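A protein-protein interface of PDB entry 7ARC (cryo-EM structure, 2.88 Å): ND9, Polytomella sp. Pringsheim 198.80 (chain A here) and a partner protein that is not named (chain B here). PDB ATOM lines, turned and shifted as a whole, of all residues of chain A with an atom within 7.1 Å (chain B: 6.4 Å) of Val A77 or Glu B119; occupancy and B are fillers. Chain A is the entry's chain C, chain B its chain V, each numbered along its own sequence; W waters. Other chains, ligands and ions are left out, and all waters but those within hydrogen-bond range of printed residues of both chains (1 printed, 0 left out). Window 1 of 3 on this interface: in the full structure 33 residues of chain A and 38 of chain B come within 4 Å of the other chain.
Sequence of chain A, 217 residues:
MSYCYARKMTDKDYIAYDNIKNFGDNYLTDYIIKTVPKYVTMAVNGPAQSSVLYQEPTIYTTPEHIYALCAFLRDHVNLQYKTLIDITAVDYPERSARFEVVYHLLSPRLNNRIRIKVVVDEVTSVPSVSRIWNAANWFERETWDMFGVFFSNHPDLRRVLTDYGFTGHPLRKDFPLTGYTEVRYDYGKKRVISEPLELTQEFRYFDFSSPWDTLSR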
ATOM      1  N   SER A   2     -24.142 -26.218   9.137  1.00  0.00           N
ATOM      2  CA  SER A   2     -23.054 -25.447   8.551  1.00  0.00           C
ATOM      3  C   SER A   2     -21.755 -26.223   8.617  1.00  0.00           C
ATOM      4  O   SER A   2     -21.554 -27.196   7.894  1.00  0.00           O
ATOM      5  CB  SER A   2     -22.902 -24.106   9.267  1.00  0.00           C
ATOM      6  OG  SER A   2     -22.488 -24.295  10.607  1.00  0.00           O
ATOM      7  N   TYR A   3     -20.865 -25.768   9.490  1.00  0.00           N
ATOM      8  CA  TYR A   3     -19.600 -26.438   9.736  1.00  0.00           C
ATOM      9  C   TYR A   3     -19.800 -27.408  10.891  1.00  0.00           C
ATOM     10  O   TYR A   3     -20.248 -27.007  11.969  1.00  0.00           O
ATOM     11  CB  TYR A   3     -18.517 -25.411  10.055  1.00  0.00           C
ATOM     12  CG  TYR A   3     -18.556 -24.231   9.115  1.00  0.00           C
ATOM     13  CD1 TYR A   3     -18.266 -24.382   7.768  1.00  0.00           C
ATOM     14  CD2 TYR A   3     -18.908 -22.970   9.570  1.00  0.00           C
ATOM     15  CE1 TYR A   3     -18.312 -23.309   6.904  1.00  0.00           C
ATOM     16  CE2 TYR A   3     -18.958 -21.892   8.713  1.00  0.00           C
ATOM     17  CZ  TYR A   3     -18.658 -22.067   7.382  1.00  0.00           C
ATOM     18  OH  TYR A   3     -18.705 -20.993   6.527  1.00  0.00           O
ATOM     19  N   PHE A  23     -36.142 -34.036   4.799  1.00  0.00           N
ATOM     20  CA  PHE A  23     -35.892 -32.891   3.928  1.00  0.00           C
ATOM     21  C   PHE A  23     -34.533 -33.070   3.261  1.00  0.00           C
ATOM     22  O   PHE A  23     -33.506 -32.543   3.692  1.00  0.00           O
ATOM     23  CB  PHE A  23     -35.957 -31.586   4.707  1.00  0.00           C
ATOM     24  CG  PHE A  23     -35.887 -30.369   3.838  1.00  0.00           C
ATOM     25  CD1 PHE A  23     -36.617 -30.300   2.664  1.00  0.00           C
ATOM     26  CD2 PHE A  23     -35.079 -29.302   4.182  1.00  0.00           C
ATOM     27  CE1 PHE A  23     -36.551 -29.186   1.858  1.00  0.00           C
ATOM     28  CE2 PHE A  23     -35.010 -28.183   3.378  1.00  0.00           C
ATOM     29  CZ  PHE A  23     -35.747 -28.127   2.215  1.00  0.00           C
ATOM     30  N   TYR A  31     -37.934 -28.935  -3.683  1.00  0.00           N
ATOM     31  CA  TYR A  31     -37.559 -27.667  -3.072  1.00  0.00           C
ATOM     32  C   TYR A  31     -36.631 -26.866  -3.973  1.00  0.00           C
ATOM     33  O   TYR A  31     -36.827 -25.661  -4.155  1.00  0.00           O
ATOM     34  CB  TYR A  31     -36.884 -27.929  -1.728  1.00  0.00           C
ATOM     35  CG  TYR A  31     -36.610 -26.700  -0.898  1.00  0.00           C
ATOM     36  CD1 TYR A  31     -37.642 -25.964  -0.335  1.00  0.00           C
ATOM     37  CD2 TYR A  31     -35.313 -26.271  -0.686  1.00  0.00           C
ATOM     38  CE1 TYR A  31     -37.379 -24.842   0.426  1.00  0.00           C
ATOM     39  CE2 TYR A  31     -35.045 -25.155   0.068  1.00  0.00           C
ATOM     40  CZ  TYR A  31     -36.076 -24.445   0.621  1.00  0.00           C
ATOM     41  OH  TYR A  31     -35.788 -23.334   1.374  1.00  0.00           O
ATOM     42  N   PHE A  72     -26.226 -20.106  -4.722  1.00  0.00           N
ATOM     43  CA  PHE A  72     -27.443 -20.426  -3.985  1.00  0.00           C
ATOM     44  C   PHE A  72     -27.277 -21.709  -3.183  1.00  0.00           C
ATOM     45  O   PHE A  72     -27.700 -21.786  -2.025  1.00  0.00           O
ATOM     46  CB  PHE A  72     -28.618 -20.545  -4.954  1.00  0.00           C
ATOM     47  CG  PHE A  72     -29.841 -21.169  -4.354  1.00  0.00           C
ATOM     48  CD1 PHE A  72     -30.644 -20.453  -3.486  1.00  0.00           C
ATOM     49  CD2 PHE A  72     -30.193 -22.471  -4.660  1.00  0.00           C
ATOM     50  CE1 PHE A  72     -31.771 -21.023  -2.936  1.00  0.00           C
ATOM     51  CE2 PHE A  72     -31.319 -23.045  -4.112  1.00  0.00           C
ATOM     52  CZ  PHE A  72     -32.108 -22.321  -3.250  1.00  0.00           C
ATOM     53  N   LEU A  73     -26.658 -22.726  -3.782  1.00  0.00           N
ATOM     54  CA  LEU A  73     -26.497 -24.006  -3.100  1.00  0.00           C
ATOM     55  C   LEU A  73     -25.591 -23.886  -1.883  1.00  0.00           C
ATOM     56  O   LEU A  73     -25.833 -24.537  -0.862  1.00  0.00           O
ATOM     57  CB  LEU A  73     -25.952 -25.056  -4.064  1.00  0.00           C
ATOM     58  CG  LEU A  73     -26.932 -25.631  -5.083  1.00  0.00           C
ATOM     59  CD1 LEU A  73     -26.207 -26.531  -6.056  1.00  0.00           C
ATOM     60  CD2 LEU A  73     -28.046 -26.384  -4.388  1.00  0.00           C
ATOM     61  N   ARG A  74     -24.531 -23.078  -1.970  1.00  0.00           N
ATOM     62  CA  ARG A  74     -23.616 -22.987  -0.836  1.00  0.00           C
ATOM     63  C   ARG A  74     -24.256 -22.293   0.360  1.00  0.00           C
ATOM     64  O   ARG A  74     -24.138 -22.768   1.494  1.00  0.00           O
ATOM     65  CB  ARG A  74     -22.350 -22.226  -1.216  1.00  0.00           C
ATOM     66  CG  ARG A  74     -21.337 -22.215  -0.082  1.00  0.00           C
ATOM     67  CD  ARG A  74     -20.074 -21.458  -0.417  1.00  0.00           C
ATOM     68  NE  ARG A  74     -20.362 -20.035  -0.560  1.00  0.00           N
ATOM     69  CZ  ARG A  74     -19.503 -19.131  -1.007  1.00  0.00           C
ATOM     70  NH1 ARG A  74     -18.256 -19.451  -1.305  1.00  0.00           N
ATOM     71  NH2 ARG A  74     -19.900 -17.869  -1.138  1.00  0.00           N
ATOM     72  N   ASP A  75     -24.943 -21.177   0.131  1.00  0.00           N
ATOM     73  CA  ASP A  75     -25.296 -20.265   1.209  1.00  0.00           C
ATOM     74  C   ASP A  75     -26.767 -20.270   1.588  1.00  0.00           C
ATOM     75  O   ASP A  75     -27.145 -19.547   2.514  1.00  0.00           O
ATOM     76  CB  ASP A  75     -24.873 -18.841   0.844  1.00  0.00           C
ATOM     77  CG  ASP A  75     -23.389 -18.611   1.026  1.00  0.00           C
ATOM     78  OD1 ASP A  75     -22.806 -19.190   1.966  1.00  0.00           O
ATOM     79  OD2 ASP A  75     -22.800 -17.853   0.229  1.00  0.00           O
ATOM     80  N   HIS A  76     -27.608 -21.047   0.915  1.00  0.00           N
ATOM     81  CA  HIS A  76     -28.995 -21.154   1.344  1.00  0.00           C
ATOM     82  C   HIS A  76     -29.075 -21.813   2.714  1.00  0.00           C
ATOM     83  O   HIS A  76     -28.350 -22.763   3.003  1.00  0.00           O
ATOM     84  CB  HIS A  76     -29.819 -21.945   0.334  1.00  0.00           C
ATOM     85  CG  HIS A  76     -31.293 -21.864   0.570  1.00  0.00           C
ATOM     86  ND1 HIS A  76     -31.965 -20.666   0.669  1.00  0.00           N
ATOM     87  CD2 HIS A  76     -32.225 -22.831   0.734  1.00  0.00           C
ATOM     88  CE1 HIS A  76     -33.248 -20.898   0.881  1.00  0.00           C
ATOM     89  NE2 HIS A  76     -33.432 -22.204   0.924  1.00  0.00           N
ATOM     90  N   VAL A  77     -29.948 -21.283   3.571  1.00  0.00           N
ATOM     91  CA  VAL A  77     -29.995 -21.741   4.958  1.00  0.00           C
ATOM     92  C   VAL A  77     -30.344 -23.225   5.020  1.00  0.00           C
ATOM     93  O   VAL A  77     -29.708 -23.999   5.743  1.00  0.00           O
ATOM     94  CB  VAL A  77     -30.976 -20.885   5.780  1.00  0.00           C
ATOM     95  CG1 VAL A  77     -30.400 -19.502   6.004  1.00  0.00           C
ATOM     96  CG2 VAL A  77     -32.320 -20.773   5.078  1.00  0.00           C
ATOM     97  N   ASN A  78     -31.360 -23.641   4.265  1.00  0.00           N
ATOM     98  CA  ASN A  78     -31.775 -25.039   4.286  1.00  0.00           C
ATOM     99  C   ASN A  78     -30.771 -25.935   3.570  1.00  0.00           C
ATOM    100  O   ASN A  78     -30.528 -27.068   4.000  1.00  0.00           O
ATOM    101  CB  ASN A  78     -33.161 -25.174   3.663  1.00  0.00           C
ATOM    102  CG  ASN A  78     -34.227 -24.460   4.465  1.00  0.00           C
ATOM    103  OD1 ASN A  78     -34.153 -24.385   5.690  1.00  0.00           O
ATOM    104  ND2 ASN A  78     -35.224 -23.923   3.775  1.00  0.00           N
ATOM    105  N   LEU A  79     -30.186 -25.452   2.478  1.00  0.00           N
ATOM    106  CA  LEU A  79     -29.224 -26.205   1.678  1.00  0.00           C
ATOM    107  C   LEU A  79     -27.858 -25.547   1.790  1.00  0.00           C
ATOM    108  O   LEU A  79     -27.621 -24.500   1.183  1.00  0.00           O
ATOM    109  CB  LEU A  79     -29.656 -26.271   0.216  1.00  0.00           C
ATOM    110  CG  LEU A  79     -30.746 -27.252  -0.187  1.00  0.00           C
ATOM    111  CD1 LEU A  79     -32.083 -26.814   0.327  1.00  0.00           C
ATOM    112  CD2 LEU A  79     -30.766 -27.348  -1.692  1.00  0.00           C
ATOM    113  N   GLN A  80     -26.957 -26.168   2.540  1.00  0.00           N
ATOM    114  CA  GLN A  80     -25.635 -25.605   2.802  1.00  0.00           C
ATOM    115  C   GLN A  80     -24.599 -26.579   2.264  1.00  0.00           C
ATOM    116  O   GLN A  80     -24.031 -27.379   3.008  1.00  0.00           O
ATOM    117  CB  GLN A  80     -25.471 -25.367   4.244  1.00  0.00           C
ATOM    118  CG  GLN A  80     -26.389 -24.297   4.741  1.00  0.00           C
ATOM    119  CD  GLN A  80     -26.260 -24.054   6.209  1.00  0.00           C
ATOM    120  OE1 GLN A  80     -25.520 -24.738   6.903  1.00  0.00           O
ATOM    121  NE2 GLN A  80     -26.983 -23.071   6.697  1.00  0.00           N
ATOM    122  N   LYS A  82     -21.399 -26.661   1.552  1.00  0.00           N
ATOM    123  CA  LYS A  82     -20.163 -25.938   1.814  1.00  0.00           C
ATOM    124  C   LYS A  82     -18.958 -26.518   1.090  1.00  0.00           C
ATOM    125  O   LYS A  82     -17.907 -25.872   1.073  1.00  0.00           O
ATOM    126  CB  LYS A  82     -19.882 -25.920   3.318  1.00  0.00           C
ATOM    127  CG  LYS A  82     -20.933 -25.200   4.134  1.00  0.00           C
ATOM    128  CD  LYS A  82     -21.234 -23.841   3.545  1.00  0.00           C
ATOM    129  CE  LYS A  82     -21.696 -22.866   4.603  1.00  0.00           C
ATOM    130  NZ  LYS A  82     -21.871 -21.505   4.033  1.00  0.00           N
ATOM    131  N   ARG A 109     -24.208 -30.153   7.025  1.00  0.00           N
ATOM    132  CA  ARG A 109     -25.402 -29.989   7.848  1.00  0.00           C
ATOM    133  C   ARG A 109     -26.484 -30.985   7.456  1.00  0.00           C
ATOM    134  O   ARG A 109     -27.101 -31.621   8.316  1.00  0.00           O
ATOM    135  CB  ARG A 109     -25.928 -28.560   7.735  1.00  0.00           C
ATOM    136  CG  ARG A 109     -27.184 -28.310   8.553  1.00  0.00           C
ATOM    137  CD  ARG A 109     -26.879 -28.396  10.046  1.00  0.00           C
ATOM    138  NE  ARG A 109     -28.048 -28.173  10.890  1.00  0.00           N
ATOM    139  CZ  ARG A 109     -28.730 -27.037  10.966  1.00  0.00           C
ATOM    140  NH1 ARG A 109     -28.385 -25.972  10.261  1.00  0.00           N
ATOM    141  NH2 ARG A 109     -29.783 -26.968  11.774  1.00  0.00           N
ATOM    142  N   LEU A 110     -26.725 -31.133   6.156  1.00  0.00           N
ATOM    143  CA  LEU A 110     -27.751 -32.040   5.667  1.00  0.00           C
ATOM    144  C   LEU A 110     -27.268 -33.475   5.554  1.00  0.00           C
ATOM    145  O   LEU A 110     -28.103 -34.369   5.382  1.00  0.00           O
ATOM    146  CB  LEU A 110     -28.260 -31.582   4.298  1.00  0.00           C
ATOM    147  CG  LEU A 110     -29.297 -30.460   4.228  1.00  0.00           C
ATOM    148  CD1 LEU A 110     -29.690 -30.213   2.783  1.00  0.00           C
ATOM    149  CD2 LEU A 110     -30.515 -30.786   5.066  1.00  0.00           C
ATOM    150  N   PHE B  61     -28.805 -14.093  18.041  1.00  0.00           N
ATOM    151  CA  PHE B  61     -29.517 -14.958  17.105  1.00  0.00           C
ATOM    152  C   PHE B  61     -30.854 -14.351  16.696  1.00  0.00           C
ATOM    153  O   PHE B  61     -31.225 -14.379  15.514  1.00  0.00           O
ATOM    154  CB  PHE B  61     -29.722 -16.334  17.740  1.00  0.00           C
ATOM    155  CG  PHE B  61     -30.118 -17.403  16.768  1.00  0.00           C
ATOM    156  CD1 PHE B  61     -29.620 -17.406  15.479  1.00  0.00           C
ATOM    157  CD2 PHE B  61     -30.985 -18.408  17.149  1.00  0.00           C
ATOM    158  CE1 PHE B  61     -29.985 -18.392  14.589  1.00  0.00           C
ATOM    159  CE2 PHE B  61     -31.352 -19.395  16.265  1.00  0.00           C
ATOM    160  CZ  PHE B  61     -30.852 -19.388  14.983  1.00  0.00           C
ATOM    161  N   LEU B  68     -32.370 -10.911   8.730  1.00  0.00           N
ATOM    162  CA  LEU B  68     -32.614 -11.696   7.524  1.00  0.00           C
ATOM    163  C   LEU B  68     -34.034 -11.489   7.012  1.00  0.00           C
ATOM    164  O   LEU B  68     -34.257 -11.362   5.800  1.00  0.00           O
ATOM    165  CB  LEU B  68     -32.357 -13.176   7.800  1.00  0.00           C
ATOM    166  CG  LEU B  68     -32.181 -14.068   6.572  1.00  0.00           C
ATOM    167  CD1 LEU B  68     -31.258 -13.410   5.562  1.00  0.00           C
ATOM    168  CD2 LEU B  68     -31.656 -15.432   6.977  1.00  0.00           C
ATOM    169  N   ALA B  84     -39.785 -19.506   1.496  1.00  0.00           N
ATOM    170  CA  ALA B  84     -38.914 -20.455   2.182  1.00  0.00           C
ATOM    171  C   ALA B  84     -38.124 -19.778   3.295  1.00  0.00           C
ATOM    172  O   ALA B  84     -38.025 -20.302   4.413  1.00  0.00           O
ATOM    173  CB  ALA B  84     -37.973 -21.112   1.177  1.00  0.00           C
ATOM    174  N   ILE B  85     -37.545 -18.610   3.005  1.00  0.00           N
ATOM    175  CA  ILE B  85     -36.769 -17.911   4.024  1.00  0.00           C
ATOM    176  C   ILE B  85     -37.667 -17.462   5.169  1.00  0.00           C
ATOM    177  O   ILE B  85     -37.287 -17.551   6.343  1.00  0.00           O
ATOM    178  CB  ILE B  85     -36.009 -16.726   3.401  1.00  0.00           C
ATOM    179  CG1 ILE B  85     -35.046 -17.223   2.328  1.00  0.00           C
ATOM    180  CG2 ILE B  85     -35.246 -15.964   4.468  1.00  0.00           C
ATOM    181  CD1 ILE B  85     -33.959 -18.116   2.870  1.00  0.00           C
ATOM    182  N   THR B  88     -38.429 -20.562   7.329  1.00  0.00           N
ATOM    183  CA  THR B  88     -37.289 -20.982   8.140  1.00  0.00           C
ATOM    184  C   THR B  88     -37.030 -20.013   9.290  1.00  0.00           C
ATOM    185  O   THR B  88     -36.786 -20.438  10.429  1.00  0.00           O
ATOM    186  CB  THR B  88     -36.045 -21.112   7.264  1.00  0.00           C
ATOM    187  OG1 THR B  88     -36.330 -21.968   6.152  1.00  0.00           O
ATOM    188  CG2 THR B  88     -34.890 -21.693   8.058  1.00  0.00           C
ATOM    189  N   ARG B  92     -37.272 -20.863  13.344  1.00  0.00           N
ATOM    190  CA  ARG B  92     -36.195 -20.669  14.312  1.00  0.00           C
ATOM    191  C   ARG B  92     -36.564 -19.646  15.378  1.00  0.00           C
ATOM    192  O   ARG B  92     -36.129 -19.773  16.528  1.00  0.00           O
ATOM    193  CB  ARG B  92     -34.889 -20.298  13.622  1.00  0.00           C
ATOM    194  CG  ARG B  92     -34.331 -21.432  12.801  1.00  0.00           C
ATOM    195  CD  ARG B  92     -33.043 -21.046  12.132  1.00  0.00           C
ATOM    196  NE  ARG B  92     -32.520 -22.140  11.328  1.00  0.00           N
ATOM    197  CZ  ARG B  92     -31.426 -22.059  10.586  1.00  0.00           C
ATOM    198  NH1 ARG B  92     -30.723 -20.942  10.516  1.00  0.00           N
ATOM    199  NH2 ARG B  92     -31.027 -23.126   9.903  1.00  0.00           N
ATOM    200  N   ALA B 111     -26.686 -27.209  16.374  1.00  0.00           N
ATOM    201  CA  ALA B 111     -25.596 -26.324  15.991  1.00  0.00           C
ATOM    202  C   ALA B 111     -25.222 -25.438  17.166  1.00  0.00           C
ATOM    203  O   ALA B 111     -26.042 -25.172  18.046  1.00  0.00           O
ATOM    204  CB  ALA B 111     -25.969 -25.470  14.777  1.00  0.00           C
ATOM    205  N   GLU B 114     -22.981 -19.729  17.636  1.00  0.00           N
ATOM    206  CA  GLU B 114     -22.129 -18.886  16.806  1.00  0.00           C
ATOM    207  C   GLU B 114     -22.335 -19.200  15.331  1.00  0.00           C
ATOM    208  O   GLU B 114     -22.478 -18.295  14.499  1.00  0.00           O
ATOM    209  CB  GLU B 114     -20.666 -19.075  17.203  1.00  0.00           C
ATOM    210  CG  GLU B 114     -20.315 -18.505  18.566  1.00  0.00           C
ATOM    211  CD  GLU B 114     -20.555 -19.489  19.695  1.00  0.00           C
ATOM    212  OE1 GLU B 114     -21.696 -19.979  19.830  1.00  0.00           O
ATOM    213  OE2 GLU B 114     -19.604 -19.771  20.452  1.00  0.00           O
ATOM    214  N   GLU B 115     -22.366 -20.488  14.989  1.00  0.00           N
ATOM    215  CA  GLU B 115     -22.538 -20.870  13.595  1.00  0.00           C
ATOM    216  C   GLU B 115     -23.978 -20.672  13.139  1.00  0.00           C
ATOM    217  O   GLU B 115     -24.219 -20.372  11.965  1.00  0.00           O
ATOM    218  CB  GLU B 115     -22.051 -22.304  13.390  1.00  0.00           C
ATOM    219  CG  GLU B 115     -22.824 -23.382  14.109  1.00  0.00           C
ATOM    220  CD  GLU B 115     -22.199 -24.746  13.899  1.00  0.00           C
ATOM    221  OE1 GLU B 115     -21.160 -24.809  13.215  1.00  0.00           O
ATOM    222  OE2 GLU B 115     -22.732 -25.748  14.417  1.00  0.00           O
ATOM    223  N   LEU B 116     -24.943 -20.794  14.055  1.00  0.00           N
ATOM    224  CA  LEU B 116     -26.314 -20.418  13.726  1.00  0.00           C
ATOM    225  C   LEU B 116     -26.404 -18.944  13.346  1.00  0.00           C
ATOM    226  O   LEU B 116     -27.134 -18.580  12.419  1.00  0.00           O
ATOM    227  CB  LEU B 116     -27.242 -20.729  14.899  1.00  0.00           C
ATOM    228  CG  LEU B 116     -27.563 -22.205  15.139  1.00  0.00           C
ATOM    229  CD1 LEU B 116     -28.170 -22.407  16.519  1.00  0.00           C
ATOM    230  CD2 LEU B 116     -28.487 -22.736  14.059  1.00  0.00           C
ATOM    231  N   ILE B 117     -25.678 -18.082  14.060  1.00  0.00           N
ATOM    232  CA  ILE B 117     -25.668 -16.661  13.725  1.00  0.00           C
ATOM    233  C   ILE B 117     -24.954 -16.423  12.400  1.00  0.00           C
ATOM    234  O   ILE B 117     -25.416 -15.634  11.567  1.00  0.00           O
ATOM    235  CB  ILE B 117     -25.039 -15.841  14.866  1.00  0.00           C
ATOM    236  CG1 ILE B 117     -25.904 -15.920  16.120  1.00  0.00           C
ATOM    237  CG2 ILE B 117     -24.851 -14.396  14.449  1.00  0.00           C
ATOM    238  CD1 ILE B 117     -25.135 -15.698  17.396  1.00  0.00           C
ATOM    239  N   ALA B 118     -23.820 -17.095  12.181  1.00  0.00           N
ATOM    240  CA  ALA B 118     -23.114 -16.949  10.911  1.00  0.00           C
ATOM    241  C   ALA B 118     -23.962 -17.425   9.737  1.00  0.00           C
ATOM    242  O   ALA B 118     -23.767 -16.969   8.603  1.00  0.00           O
ATOM    243  CB  ALA B 118     -21.792 -17.713  10.953  1.00  0.00           C
ATOM    244  N   GLU B 119     -24.896 -18.342   9.993  1.00  0.00           N
ATOM    245  CA  GLU B 119     -25.754 -18.871   8.939  1.00  0.00           C
ATOM    246  C   GLU B 119     -26.575 -17.771   8.273  1.00  0.00           C
ATOM    247  O   GLU B 119     -26.696 -17.728   7.043  1.00  0.00           O
ATOM    248  CB  GLU B 119     -26.671 -19.941   9.526  1.00  0.00           C
ATOM    249  CG  GLU B 119     -27.587 -20.595   8.528  1.00  0.00           C
ATOM    250  CD  GLU B 119     -28.200 -21.869   9.069  1.00  0.00           C
ATOM    251  OE1 GLU B 119     -27.656 -22.424  10.047  1.00  0.00           O
ATOM    252  OE2 GLU B 119     -29.218 -22.324   8.507  1.00  0.00           O
ATOM    253  N   SER B 120     -27.164 -16.881   9.073  1.00  0.00           N
ATOM    254  CA  SER B 120     -28.004 -15.834   8.501  1.00  0.00           C
ATOM    255  C   SER B 120     -27.182 -14.841   7.687  1.00  0.00           C
ATOM    256  O   SER B 120     -27.642 -14.353   6.651  1.00  0.00           O
ATOM    257  CB  SER B 120     -28.769 -15.118   9.612  1.00  0.00           C
ATOM    258  OG  SER B 120     -29.661 -16.006  10.258  1.00  0.00           O
ATOM    259  N   LYS B 121     -25.964 -14.533   8.131  1.00  0.00           N
ATOM    260  CA  LYS B 121     -25.093 -13.669   7.339  1.00  0.00           C
ATOM    261  C   LYS B 121     -24.709 -14.336   6.022  1.00  0.00           C
ATOM    262  O   LYS B 121     -24.672 -13.684   4.966  1.00  0.00           O
ATOM    263  CB  LYS B 121     -23.851 -13.308   8.148  1.00  0.00           C
ATOM    264  CG  LYS B 121     -24.157 -12.454   9.361  1.00  0.00           C
ATOM    265  CD  LYS B 121     -22.900 -12.100  10.130  1.00  0.00           C
ATOM    266  CE  LYS B 121     -23.225 -11.177  11.288  1.00  0.00           C
ATOM    267  NZ  LYS B 121     -24.048 -11.868  12.317  1.00  0.00           N
ATOM    268  N   GLU B 122     -24.425 -15.639   6.066  1.00  0.00           N
ATOM    269  CA  GLU B 122     -24.117 -16.367   4.841  1.00  0.00           C
ATOM    270  C   GLU B 122     -25.299 -16.343   3.885  1.00  0.00           C
ATOM    271  O   GLU B 122     -25.123 -16.227   2.667  1.00  0.00           O
ATOM    272  CB  GLU B 122     -23.737 -17.807   5.182  1.00  0.00           C
ATOM    273  CG  GLU B 122     -22.435 -17.937   5.952  1.00  0.00           C
ATOM    274  CD  GLU B 122     -22.096 -19.372   6.290  1.00  0.00           C
ATOM    275  OE1 GLU B 122     -22.939 -20.257   6.036  1.00  0.00           O
ATOM    276  OE2 GLU B 122     -20.987 -19.614   6.812  1.00  0.00           O
ATOM    277  N   GLU B 123     -26.515 -16.440   4.421  1.00  0.00           N
ATOM    278  CA  GLU B 123     -27.708 -16.260   3.600  1.00  0.00           C
ATOM    279  C   GLU B 123     -27.776 -14.853   3.021  1.00  0.00           C
ATOM    280  O   GLU B 123     -28.163 -14.663   1.864  1.00  0.00           O
ATOM    281  CB  GLU B 123     -28.958 -16.541   4.431  1.00  0.00           C
ATOM    282  CG  GLU B 123     -30.261 -16.420   3.665  1.00  0.00           C
ATOM    283  CD  GLU B 123     -30.391 -17.457   2.577  1.00  0.00           C
ATOM    284  OE1 GLU B 123     -29.767 -18.525   2.710  1.00  0.00           O
ATOM    285  OE2 GLU B 123     -31.111 -17.207   1.589  1.00  0.00           O
ATOM    286  N   LEU B 124     -27.411 -13.856   3.826  1.00  0.00           N
ATOM    287  CA  LEU B 124     -27.396 -12.471   3.373  1.00  0.00           C
ATOM    288  C   LEU B 124     -26.442 -12.243   2.205  1.00  0.00           C
ATOM    289  O   LEU B 124     -26.703 -11.375   1.364  1.00  0.00           O
ATOM    290  CB  LEU B 124     -27.048 -11.555   4.544  1.00  0.00           C
ATOM    291  CG  LEU B 124     -27.045 -10.052   4.285  1.00  0.00           C
ATOM    292  CD1 LEU B 124     -28.434  -9.591   3.891  1.00  0.00           C
ATOM    293  CD2 LEU B 124     -26.566  -9.310   5.521  1.00  0.00           C
ATOM    294  N   ILE B 126     -25.785 -13.893  -0.501  1.00  0.00           N
ATOM    295  CA  ILE B 126     -26.234 -14.261  -1.842  1.00  0.00           C
ATOM    296  C   ILE B 126     -27.509 -13.560  -2.278  1.00  0.00           C
ATOM    297  O   ILE B 126     -27.962 -13.784  -3.409  1.00  0.00           O
ATOM    298  CB  ILE B 126     -26.448 -15.783  -1.968  1.00  0.00           C
ATOM    299  CG1 ILE B 126     -27.539 -16.247  -1.003  1.00  0.00           C
ATOM    300  CG2 ILE B 126     -25.142 -16.517  -1.748  1.00  0.00           C
ATOM    301  CD1 ILE B 126     -27.981 -17.672  -1.214  1.00  0.00           C
HETATM  302  O   HOH W   1     -33.211 -25.150   8.682  1.00  0.00           O
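Of the 19 printed residues of chain B, 9 touch a printed residue of chain A. Printed residues of chain B that touch a printed residue of chain A: Ala B84, Ile B85, Thr B88, Arg B92, Glu B115, Glu B119, Glu B122, Glu B123 and Ile B126. Hydrophobic or aromatic side chains of chain A within 4 Å of the printed part of chain B: Tyr A3, Tyr A31, His A76 and Val A77.
NE2 of Gln A80 lies close to OE2 of Glu B119 (3.0 Å). The backbone carbonyl oxygen (O) of Tyr A3 sits close to the side-chain carboxylate (OE1) of Glu B115, 2.7 Å away. The side-chain carboxylate (OE1) of Glu B122 is in salt-bridge range of the side-chain amino group (NZ) of Lys A82, at 2.6 Å. The side-chain hydroxyl of Thr B88 sits at hydrogen-bond distance from the side-chain amide nitrogen of Asn A78 (3.3 Å). The side-chain carboxylate of Glu B122 sits at hydrogen-bond distance from the side-chain hydroxyl of Tyr A3, at 2.7 Å. The side-chain carboxylate of Glu B123 sits at hydrogen-bond distance from the backbone NH of Val A77, 2.9 Å away. The side-chain carboxylate of Glu B119 lies within salt-bridge range of the guanidinium group of Arg A109 (3.6 Å). O of Asp A75 sits close to OE1 of Glu B123 (2.8 Å). The backbone carbonyl oxygen (O) of Val A77 sits close to the side-chain carboxylate (OE2) of Glu B119 (3.3 Å). The side-chain carboxylate of Glu B115 is in hydrogen-bond range of the side-chain hydroxyl of Ser A2.
The side-chain hydroxyl (OH) of Tyr A31 lies within hydrogen-bond range of a ring nitrogen (NE2) of His A76. The backbone carbonyl oxygen of Ala B84 lies within hydrogen-bond range of the side-chain hydroxyl of Thr B88 (2.9 Å). The side-chain amide nitrogen (NE2) of Gln A80 sits at hydrogen-bond distance from the backbone carbonyl oxygen (O) of Val A77 (3.0 Å). NH2 of Arg A74 lies within salt-bridge range of OD2 of Asp A75, 3.2 Å away. N of Ser A2 lies within hydrogen-bond range of OE1 of Gln A80. NH2 of Arg B92 lies within salt-bridge range of OE2 of Glu B119 (2.4 Å).
Water W1 lies within hydrogen-bond range of the guanidinium group (NH2) of Arg B92 and the side-chain amide oxygen (OD1) of Asn A78.
Tyr A31 touches Ala B84. CA of Phe A72 touches CD1 of Ile B126, at 3.9 Å. Asp A75 touches Glu B122 (CB to O, 3.2 Å). CG2 of Ile B126 touches OD2 of Asp A75 (3.3 Å). CE1 of His A76 touches CD1 of Ile B85 (3.5 Å). His A76 touches Glu B123. Val A77 touches Ile B85 (CG2 to CD1, 3.8 Å). NH1 of Arg A109 touches NH2 of Arg B92, at 3.9 Å.
Of chain B, only Ile B85 (3.8 Å), Glu B119 (3.3 Å) and Glu B123 (2.9 Å) come within 4 Å of Val A77. Glu B119 touches three residues of chain A. Printed residues of chain B within 4 Å of Tyr A3: Glu B115 and Glu B122. Of the printed residues of chain A, Ile B85 touches His A76 (3.5 Å) and Val A77 (3.8 Å). Printed residues of chain B within 4 Å of Ser A2: Glu B115 (3.0 Å). The nearest residue of chain B that does not touch Val A77 is Thr B88 (4.04 Å). The nearest residue of chain A that does not touch Glu B119 is Asp A75 (4.9 Å). The nearest printed residue of chain A that does not touch Ala B84 is Asn A78 (4.6 Å).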
